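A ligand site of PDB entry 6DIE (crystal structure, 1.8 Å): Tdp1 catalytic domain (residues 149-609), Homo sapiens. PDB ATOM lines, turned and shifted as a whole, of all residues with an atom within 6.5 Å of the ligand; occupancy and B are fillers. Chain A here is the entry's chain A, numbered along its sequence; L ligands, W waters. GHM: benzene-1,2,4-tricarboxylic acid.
NE2 of His 346 lies within hydrogen-bond range of O3 of the ligand. The side-chain amino group of Lys 348 lies within salt-bridge range of an oxygen (O6) of the ligand (2.7 Å). The side-chain amide nitrogen (ND2) of Asn 369 is in hydrogen-bond range of an oxygen (O5) of the ligand, at 3.1 Å. The side-chain amide nitrogen of Asn 136 sits at hydrogen-bond distance from an oxygen (O3) of the ligand (2.8 Å). The side-chain hydroxyl (OG) of Ser 252 lies within hydrogen-bond range of an oxygen (O5) of the ligand, at 2.6 Å. O4 of the ligand lies within salt-bridge range of NZ of Lys 118. An oxygen (O4) of the ligand lies within hydrogen-bond range of a ring nitrogen (ND1) of His 116 (3.1 Å). An oxygen (O2) of the ligand is in hydrogen-bond range of the side-chain hydroxyl of Ser 253.
The side-chain amide oxygen of Asn 369 sits at hydrogen-bond distance from the backbone NH of Ser 253 (3.1 Å). The side-chain amino group of Lys 118 sits at hydrogen-bond distance from the backbone carbonyl oxygen of His 116 (2.8 Å). N of Asn 136 sits at hydrogen-bond distance from OD2 of Asp 141 (2.8 Å). ND1 of His 346 lies within hydrogen-bond range of O of Thr 134 (2.8 Å). O of His 346 is in hydrogen-bond range of NZ of Lys 348 (2.7 Å). The backbone carbonyl oxygen (O) of Pro 314 lies within hydrogen-bond range of the side-chain hydroxyl (OG) of Ser 253 (3.3 Å). The side-chain hydroxyl (OG) of Ser 252 sits at hydrogen-bond distance from the side-chain amino group (NZ) of Lys 348, at 3.1 Å. OD1 of Asn 136 lies within hydrogen-bond range of N of Cys 58 (3.0 Å).
Tyr 57 touches the ligand (CB to O4, 3.4 Å). CG of Pro 314 touches O2 of the ligand, at 3.5 Å. Of the 23 residues printed, 10 come within 4 Å of the ligand.
Water W1 lies within hydrogen-bond range of an oxygen (O6) of the ligand (2.5 Å), the backbone carbonyl oxygen of Ser 367 (2.8 Å), a ring nitrogen (ND1) of His 116 (3.3 Å) and the side-chain amino group of Lys 118 (3.5 Å). Water W3 lies within hydrogen-bond range of an oxygen (O2) of the ligand (2.6 Å), the side-chain hydroxyl (OG) of Ser 253 (2.8 Å) and the backbone carbonyl oxygen (O) of Pro 314 (2.9 Å). Water W4 lies within hydrogen-bond range of an oxygen (O5) of the ligand (3.1 Å), the backbone carbonyl oxygen (O) of Ser 312 (3.2 Å) and a ring nitrogen (NE2) of His 346 (3.5 Å).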
ATOM      1  N   ASN A  56     -26.250  -7.996  -4.959  1.00  0.00           N
ATOM      2  CA  ASN A  56     -25.229  -6.957  -4.889  1.00  0.00           C
ATOM      3  C   ASN A  56     -25.855  -5.610  -5.231  1.00  0.00           C
ATOM      4  O   ASN A  56     -27.072  -5.473  -5.375  1.00  0.00           O
ATOM      5  CB  ASN A  56     -24.038  -7.267  -5.797  1.00  0.00           C
ATOM      6  CG  ASN A  56     -22.722  -6.859  -5.145  1.00  0.00           C
ATOM      7  OD1 ASN A  56     -22.479  -5.682  -4.928  1.00  0.00           O
ATOM      8  ND2 ASN A  56     -21.886  -7.841  -4.794  1.00  0.00           N
ATOM      9  N   TYR A  57     -24.987  -4.601  -5.352  1.00  0.00           N
ATOM     10  CA  TYR A  57     -25.377  -3.248  -5.711  1.00  0.00           C
ATOM     11  C   TYR A  57     -24.959  -2.917  -7.132  1.00  0.00           C
ATOM     12  O   TYR A  57     -25.805  -2.554  -7.975  1.00  0.00           O
ATOM     13  CB  TYR A  57     -24.755  -2.251  -4.715  1.00  0.00           C
ATOM     14  CG  TYR A  57     -24.908  -0.817  -5.155  1.00  0.00           C
ATOM     15  CD1 TYR A  57     -26.136  -0.173  -5.052  1.00  0.00           C
ATOM     16  CD2 TYR A  57     -23.840  -0.121  -5.701  1.00  0.00           C
ATOM     17  CE1 TYR A  57     -26.289   1.143  -5.478  1.00  0.00           C
ATOM     18  CE2 TYR A  57     -23.989   1.187  -6.130  1.00  0.00           C
ATOM     19  CZ  TYR A  57     -25.206   1.811  -6.018  1.00  0.00           C
ATOM     20  OH  TYR A  57     -25.331   3.105  -6.438  1.00  0.00           O
ATOM     21  N   CYS A  58     -23.672  -3.070  -7.448  1.00  0.00           N
ATOM     22  CA  CYS A  58     -23.106  -2.763  -8.749  1.00  0.00           C
ATOM     23  C   CYS A  58     -22.545  -4.023  -9.379  1.00  0.00           C
ATOM     24  O   CYS A  58     -21.852  -4.796  -8.716  1.00  0.00           O
ATOM     25  CB  CYS A  58     -22.009  -1.687  -8.623  1.00  0.00           C
ATOM     26  SG  CYS A  58     -21.405  -1.078 -10.202  1.00  0.00           S
ATOM     27  N   THR A 114     -31.545   1.804  -0.976  1.00  0.00           N
ATOM     28  CA  THR A 114     -30.594   1.149  -1.848  1.00  0.00           C
ATOM     29  C   THR A 114     -30.621  -0.342  -1.540  1.00  0.00           C
ATOM     30  O   THR A 114     -30.971  -0.737  -0.426  1.00  0.00           O
ATOM     31  CB  THR A 114     -29.185   1.745  -1.647  1.00  0.00           C
ATOM     32  OG1 THR A 114     -29.210   3.150  -1.891  1.00  0.00           O
ATOM     33  CG2 THR A 114     -28.172   1.098  -2.566  1.00  0.00           C
ATOM     34  N   HIS A 115     -30.264  -1.163  -2.527  1.00  0.00           N
ATOM     35  CA  HIS A 115     -30.019  -2.587  -2.272  1.00  0.00           C
ATOM     36  C   HIS A 115     -28.516  -2.790  -2.114  1.00  0.00           C
ATOM     37  O   HIS A 115     -27.791  -2.983  -3.094  1.00  0.00           O
ATOM     38  CB  HIS A 115     -30.586  -3.459  -3.386  1.00  0.00           C
ATOM     39  CG  HIS A 115     -30.432  -4.920  -3.118  1.00  0.00           C
ATOM     40  ND1 HIS A 115     -29.360  -5.646  -3.586  1.00  0.00           N
ATOM     41  CD2 HIS A 115     -31.190  -5.785  -2.416  1.00  0.00           C
ATOM     42  CE1 HIS A 115     -29.471  -6.893  -3.184  1.00  0.00           C
ATOM     43  NE2 HIS A 115     -30.575  -7.008  -2.469  1.00  0.00           N
ATOM     44  N   HIS A 116     -28.023  -2.739  -0.874  1.00  0.00           N
ATOM     45  CA  HIS A 116     -26.572  -2.813  -0.651  1.00  0.00           C
ATOM     46  C   HIS A 116     -26.089  -4.219  -0.354  1.00  0.00           C
ATOM     47  O   HIS A 116     -24.891  -4.475  -0.470  1.00  0.00           O
ATOM     48  CB  HIS A 116     -26.128  -1.950   0.537  1.00  0.00           C
ATOM     49  CG  HIS A 116     -26.120  -0.471   0.290  1.00  0.00           C
ATOM     50  ND1 HIS A 116     -25.227   0.132  -0.562  1.00  0.00           N
ATOM     51  CD2 HIS A 116     -26.837   0.522   0.856  1.00  0.00           C
ATOM     52  CE1 HIS A 116     -25.435   1.443  -0.556  1.00  0.00           C
ATOM     53  NE2 HIS A 116     -26.412   1.700   0.301  1.00  0.00           N
ATOM     54  N   THR A 117     -26.974  -5.120   0.091  1.00  0.00           N
ATOM     55  CA  THR A 117     -26.574  -6.486   0.476  1.00  0.00           C
ATOM     56  C   THR A 117     -25.661  -7.135  -0.547  1.00  0.00           C
ATOM     57  O   THR A 117     -25.924  -7.081  -1.753  1.00  0.00           O
ATOM     58  CB  THR A 117     -27.833  -7.336   0.647  1.00  0.00           C
ATOM     59  OG1 THR A 117     -28.573  -6.827   1.754  1.00  0.00           O
ATOM     60  CG2 THR A 117     -27.479  -8.804   0.881  1.00  0.00           C
ATOM     61  N   LYS A 118     -24.573  -7.738  -0.063  1.00  0.00           N
ATOM     62  CA  LYS A 118     -23.641  -8.488  -0.907  1.00  0.00           C
ATOM     63  C   LYS A 118     -23.573  -9.925  -0.393  1.00  0.00           C
ATOM     64  O   LYS A 118     -23.098 -10.193   0.712  1.00  0.00           O
ATOM     65  CB  LYS A 118     -22.285  -7.799  -0.923  1.00  0.00           C
ATOM     66  CG  LYS A 118     -22.450  -6.423  -1.572  1.00  0.00           C
ATOM     67  CD  LYS A 118     -21.452  -5.458  -1.049  1.00  0.00           C
ATOM     68  CE  LYS A 118     -21.449  -4.191  -1.900  1.00  0.00           C
ATOM     69  NZ  LYS A 118     -22.564  -3.310  -1.502  1.00  0.00           N
ATOM     70  N   THR A 134     -18.481  -7.964   1.282  1.00  0.00           N
ATOM     71  CA  THR A 134     -18.631  -6.517   1.179  1.00  0.00           C
ATOM     72  C   THR A 134     -18.321  -5.929  -0.207  1.00  0.00           C
ATOM     73  O   THR A 134     -18.383  -4.703  -0.351  1.00  0.00           O
ATOM     74  CB  THR A 134     -17.757  -5.804   2.216  1.00  0.00           C
ATOM     75  OG1 THR A 134     -16.365  -6.092   1.969  1.00  0.00           O
ATOM     76  CG2 THR A 134     -18.116  -6.243   3.639  1.00  0.00           C
ATOM     77  N   SER A 135     -18.033  -6.746  -1.208  1.00  0.00           N
ATOM     78  CA  SER A 135     -17.507  -6.269  -2.492  1.00  0.00           C
ATOM     79  C   SER A 135     -18.570  -6.221  -3.567  1.00  0.00           C
ATOM     80  O   SER A 135     -19.344  -7.172  -3.733  1.00  0.00           O
ATOM     81  CB  SER A 135     -16.374  -7.176  -2.983  1.00  0.00           C
ATOM     82  OG  SER A 135     -15.305  -7.209  -2.052  1.00  0.00           O
ATOM     83  N   ASN A 136     -18.599  -5.129  -4.327  1.00  0.00           N
ATOM     84  CA  ASN A 136     -19.369  -5.094  -5.550  1.00  0.00           C
ATOM     85  C   ASN A 136     -18.779  -6.076  -6.570  1.00  0.00           C
ATOM     86  O   ASN A 136     -17.630  -6.489  -6.464  1.00  0.00           O
ATOM     87  CB  ASN A 136     -19.393  -3.678  -6.127  1.00  0.00           C
ATOM     88  CG  ASN A 136     -20.249  -2.739  -5.287  1.00  0.00           C
ATOM     89  OD1 ASN A 136     -21.474  -2.756  -5.378  1.00  0.00           O
ATOM     90  ND2 ASN A 136     -19.599  -1.935  -4.432  1.00  0.00           N
ATOM     91  N   ASP A 141     -13.365  -3.517  -7.154  1.00  0.00           N
ATOM     92  CA  ASP A 141     -13.637  -3.805  -5.749  1.00  0.00           C
ATOM     93  C   ASP A 141     -12.820  -4.984  -5.233  1.00  0.00           C
ATOM     94  O   ASP A 141     -12.711  -5.155  -4.005  1.00  0.00           O
ATOM     95  CB  ASP A 141     -15.133  -4.062  -5.543  1.00  0.00           C
ATOM     96  CG  ASP A 141     -15.868  -2.829  -5.064  1.00  0.00           C
ATOM     97  OD1 ASP A 141     -15.539  -1.726  -5.552  1.00  0.00           O
ATOM     98  OD2 ASP A 141     -16.766  -2.959  -4.189  1.00  0.00           O
ATOM     99  N   SER A 252     -17.234   2.925   4.919  1.00  0.00           N
ATOM    100  CA  SER A 252     -16.769   3.582   3.709  1.00  0.00           C
ATOM    101  C   SER A 252     -17.636   4.758   3.290  1.00  0.00           C
ATOM    102  O   SER A 252     -17.295   5.466   2.330  1.00  0.00           O
ATOM    103  CB  SER A 252     -16.658   2.563   2.563  1.00  0.00           C
ATOM    104  OG  SER A 252     -17.921   1.985   2.255  1.00  0.00           O
ATOM    105  N   SER A 253     -18.744   5.012   3.984  1.00  0.00           N
ATOM    106  CA  SER A 253     -19.536   6.202   3.712  1.00  0.00           C
ATOM    107  C   SER A 253     -20.330   6.560   4.961  1.00  0.00           C
ATOM    108  O   SER A 253     -20.478   5.752   5.883  1.00  0.00           O
ATOM    109  CB  SER A 253     -20.476   6.019   2.521  1.00  0.00           C
ATOM    110  OG  SER A 253     -20.927   7.284   2.074  1.00  0.00           O
ATOM    111  N   VAL A 254     -20.820   7.803   5.000  1.00  0.00           N
ATOM    112  CA  VAL A 254     -21.582   8.343   6.123  1.00  0.00           C
ATOM    113  C   VAL A 254     -22.789   9.057   5.547  1.00  0.00           C
ATOM    114  O   VAL A 254     -22.668   9.796   4.570  1.00  0.00           O
ATOM    115  CB  VAL A 254     -20.754   9.327   6.982  1.00  0.00           C
ATOM    116  CG1 VAL A 254     -21.434   9.523   8.332  1.00  0.00           C
ATOM    117  CG2 VAL A 254     -19.322   8.861   7.132  1.00  0.00           C
ATOM    118  N   SER A 312     -14.899   5.241  -4.311  1.00  0.00           N
ATOM    119  CA  SER A 312     -15.627   4.247  -3.532  1.00  0.00           C
ATOM    120  C   SER A 312     -15.745   4.626  -2.065  1.00  0.00           C
ATOM    121  O   SER A 312     -16.025   3.759  -1.220  1.00  0.00           O
ATOM    122  CB  SER A 312     -14.981   2.867  -3.678  1.00  0.00           C
ATOM    123  OG  SER A 312     -15.059   2.431  -5.026  1.00  0.00           O
ATOM    124  N   LEU A 313     -15.525   5.903  -1.742  1.00  0.00           N
ATOM    125  CA  LEU A 313     -15.738   6.460  -0.406  1.00  0.00           C
ATOM    126  C   LEU A 313     -16.652   7.665  -0.565  1.00  0.00           C
ATOM    127  O   LEU A 313     -16.203   8.817  -0.480  1.00  0.00           O
ATOM    128  CB  LEU A 313     -14.411   6.849   0.255  1.00  0.00           C
ATOM    129  CG  LEU A 313     -13.404   5.710   0.470  1.00  0.00           C
ATOM    130  CD1 LEU A 313     -11.951   6.216   0.518  1.00  0.00           C
ATOM    131  CD2 LEU A 313     -13.739   4.897   1.741  1.00  0.00           C
ATOM    132  N   PRO A 314     -17.934   7.442  -0.819  1.00  0.00           N
ATOM    133  CA  PRO A 314     -18.814   8.505  -1.361  1.00  0.00           C
ATOM    134  C   PRO A 314     -19.443   9.402  -0.309  1.00  0.00           C
ATOM    135  O   PRO A 314     -20.660   9.571  -0.253  1.00  0.00           O
ATOM    136  CB  PRO A 314     -19.862   7.698  -2.129  1.00  0.00           C
ATOM    137  CG  PRO A 314     -19.947   6.420  -1.402  1.00  0.00           C
ATOM    138  CD  PRO A 314     -18.591   6.124  -0.827  1.00  0.00           C
ATOM    139  N   TYR A 315     -18.604  10.036   0.506  1.00  0.00           N
ATOM    140  CA  TYR A 315     -19.035  11.027   1.487  1.00  0.00           C
ATOM    141  C   TYR A 315     -19.075  12.384   0.789  1.00  0.00           C
ATOM    142  O   TYR A 315     -18.030  12.897   0.388  1.00  0.00           O
ATOM    143  CB  TYR A 315     -18.077  11.024   2.678  1.00  0.00           C
ATOM    144  CG  TYR A 315     -18.506  11.797   3.905  1.00  0.00           C
ATOM    145  CD1 TYR A 315     -19.844  12.103   4.143  1.00  0.00           C
ATOM    146  CD2 TYR A 315     -17.565  12.217   4.822  1.00  0.00           C
ATOM    147  CE1 TYR A 315     -20.219  12.797   5.283  1.00  0.00           C
ATOM    148  CE2 TYR A 315     -17.928  12.906   5.966  1.00  0.00           C
ATOM    149  CZ  TYR A 315     -19.255  13.200   6.179  1.00  0.00           C
ATOM    150  OH  TYR A 315     -19.606  13.882   7.327  1.00  0.00           O
ATOM    151  N   HIS A 346     -13.281  -0.916   1.831  1.00  0.00           N
ATOM    152  CA  HIS A 346     -14.684  -0.954   1.459  1.00  0.00           C
ATOM    153  C   HIS A 346     -15.439  -1.950   2.338  1.00  0.00           C
ATOM    154  O   HIS A 346     -16.670  -2.030   2.261  1.00  0.00           O
ATOM    155  CB  HIS A 346     -14.821  -1.302  -0.047  1.00  0.00           C
ATOM    156  CG  HIS A 346     -16.217  -1.208  -0.576  1.00  0.00           C
ATOM    157  ND1 HIS A 346     -17.068  -2.292  -0.629  1.00  0.00           N
ATOM    158  CD2 HIS A 346     -16.897  -0.178  -1.141  1.00  0.00           C
ATOM    159  CE1 HIS A 346     -18.223  -1.927  -1.169  1.00  0.00           C
ATOM    160  NE2 HIS A 346     -18.141  -0.647  -1.481  1.00  0.00           N
ATOM    161  N   LYS A 348     -17.017  -2.950   5.958  1.00  0.00           N
ATOM    162  CA  LYS A 348     -17.604  -2.254   7.083  1.00  0.00           C
ATOM    163  C   LYS A 348     -17.573  -3.198   8.277  1.00  0.00           C
ATOM    164  O   LYS A 348     -17.955  -4.370   8.133  1.00  0.00           O
ATOM    165  CB  LYS A 348     -19.059  -1.812   6.839  1.00  0.00           C
ATOM    166  CG  LYS A 348     -19.205  -0.821   5.689  1.00  0.00           C
ATOM    167  CD  LYS A 348     -19.448  -1.563   4.368  1.00  0.00           C
ATOM    168  CE  LYS A 348     -19.843  -0.575   3.282  1.00  0.00           C
ATOM    169  NZ  LYS A 348     -19.130  -0.856   2.022  1.00  0.00           N
ATOM    170  N   SER A 367     -22.533  -5.039   5.224  1.00  0.00           N
ATOM    171  CA  SER A 367     -22.591  -4.040   4.174  1.00  0.00           C
ATOM    172  C   SER A 367     -22.950  -2.654   4.700  1.00  0.00           C
ATOM    173  O   SER A 367     -22.797  -1.672   3.969  1.00  0.00           O
ATOM    174  CB  SER A 367     -23.642  -4.450   3.126  1.00  0.00           C
ATOM    175  OG  SER A 367     -24.924  -4.572   3.738  1.00  0.00           O
ATOM    176  N   ASN A 369     -23.126   0.892   6.081  1.00  0.00           N
ATOM    177  CA  ASN A 369     -22.339   2.086   6.402  1.00  0.00           C
ATOM    178  C   ASN A 369     -22.949   2.825   7.588  1.00  0.00           C
ATOM    179  O   ASN A 369     -23.964   2.420   8.172  1.00  0.00           O
ATOM    180  CB  ASN A 369     -22.264   2.988   5.173  1.00  0.00           C
ATOM    181  CG  ASN A 369     -21.153   2.597   4.248  1.00  0.00           C
ATOM    182  OD1 ASN A 369     -20.063   2.256   4.695  1.00  0.00           O
ATOM    183  ND2 ASN A 369     -21.419   2.637   2.953  1.00  0.00           N
HETATM  184  C4  GHM L   1     -23.197   2.057  -2.863  1.00  0.00           C
HETATM  185  C5  GHM L   1     -22.261   1.483  -2.003  1.00  0.00           C
HETATM  186  C6  GHM L   1     -21.857   0.050  -2.240  1.00  0.00           C
HETATM  187  C7  GHM L   1     -21.692   2.233  -0.994  1.00  0.00           C
HETATM  188  C8  GHM L   1     -20.691   1.648  -0.046  1.00  0.00           C
HETATM  189  C9  GHM L   1     -22.099   3.551  -0.809  1.00  0.00           C
HETATM  190  C3  GHM L   1     -23.586   3.386  -2.688  1.00  0.00           C
HETATM  191  C1  GHM L   1     -23.441   5.560  -1.446  1.00  0.00           C
HETATM  192  C2  GHM L   1     -23.048   4.126  -1.652  1.00  0.00           C
HETATM  193  O1  GHM L   1     -23.922   6.222  -2.350  1.00  0.00           O
HETATM  194  O2  GHM L   1     -23.271   6.136  -0.250  1.00  0.00           O
HETATM  195  O3  GHM L   1     -20.708  -0.268  -2.434  1.00  0.00           O
HETATM  196  O4  GHM L   1     -22.810  -0.877  -2.257  1.00  0.00           O
HETATM  197  O5  GHM L   1     -19.715   2.270   0.340  1.00  0.00           O
HETATM  198  O6  GHM L   1     -20.879   0.425   0.426  1.00  0.00           O
HETATM  199  O   HOH W   1     -22.744  -1.098   1.200  1.00  0.00           O
HETATM  200  O   HOH W   2     -24.032   8.798  -2.079  1.00  0.00           O
HETATM  201  O   HOH W   3     -23.130   8.458   0.889  1.00  0.00           O
HETATM  202  O   HOH W   4     -18.688   2.596  -2.565  1.00  0.00           O
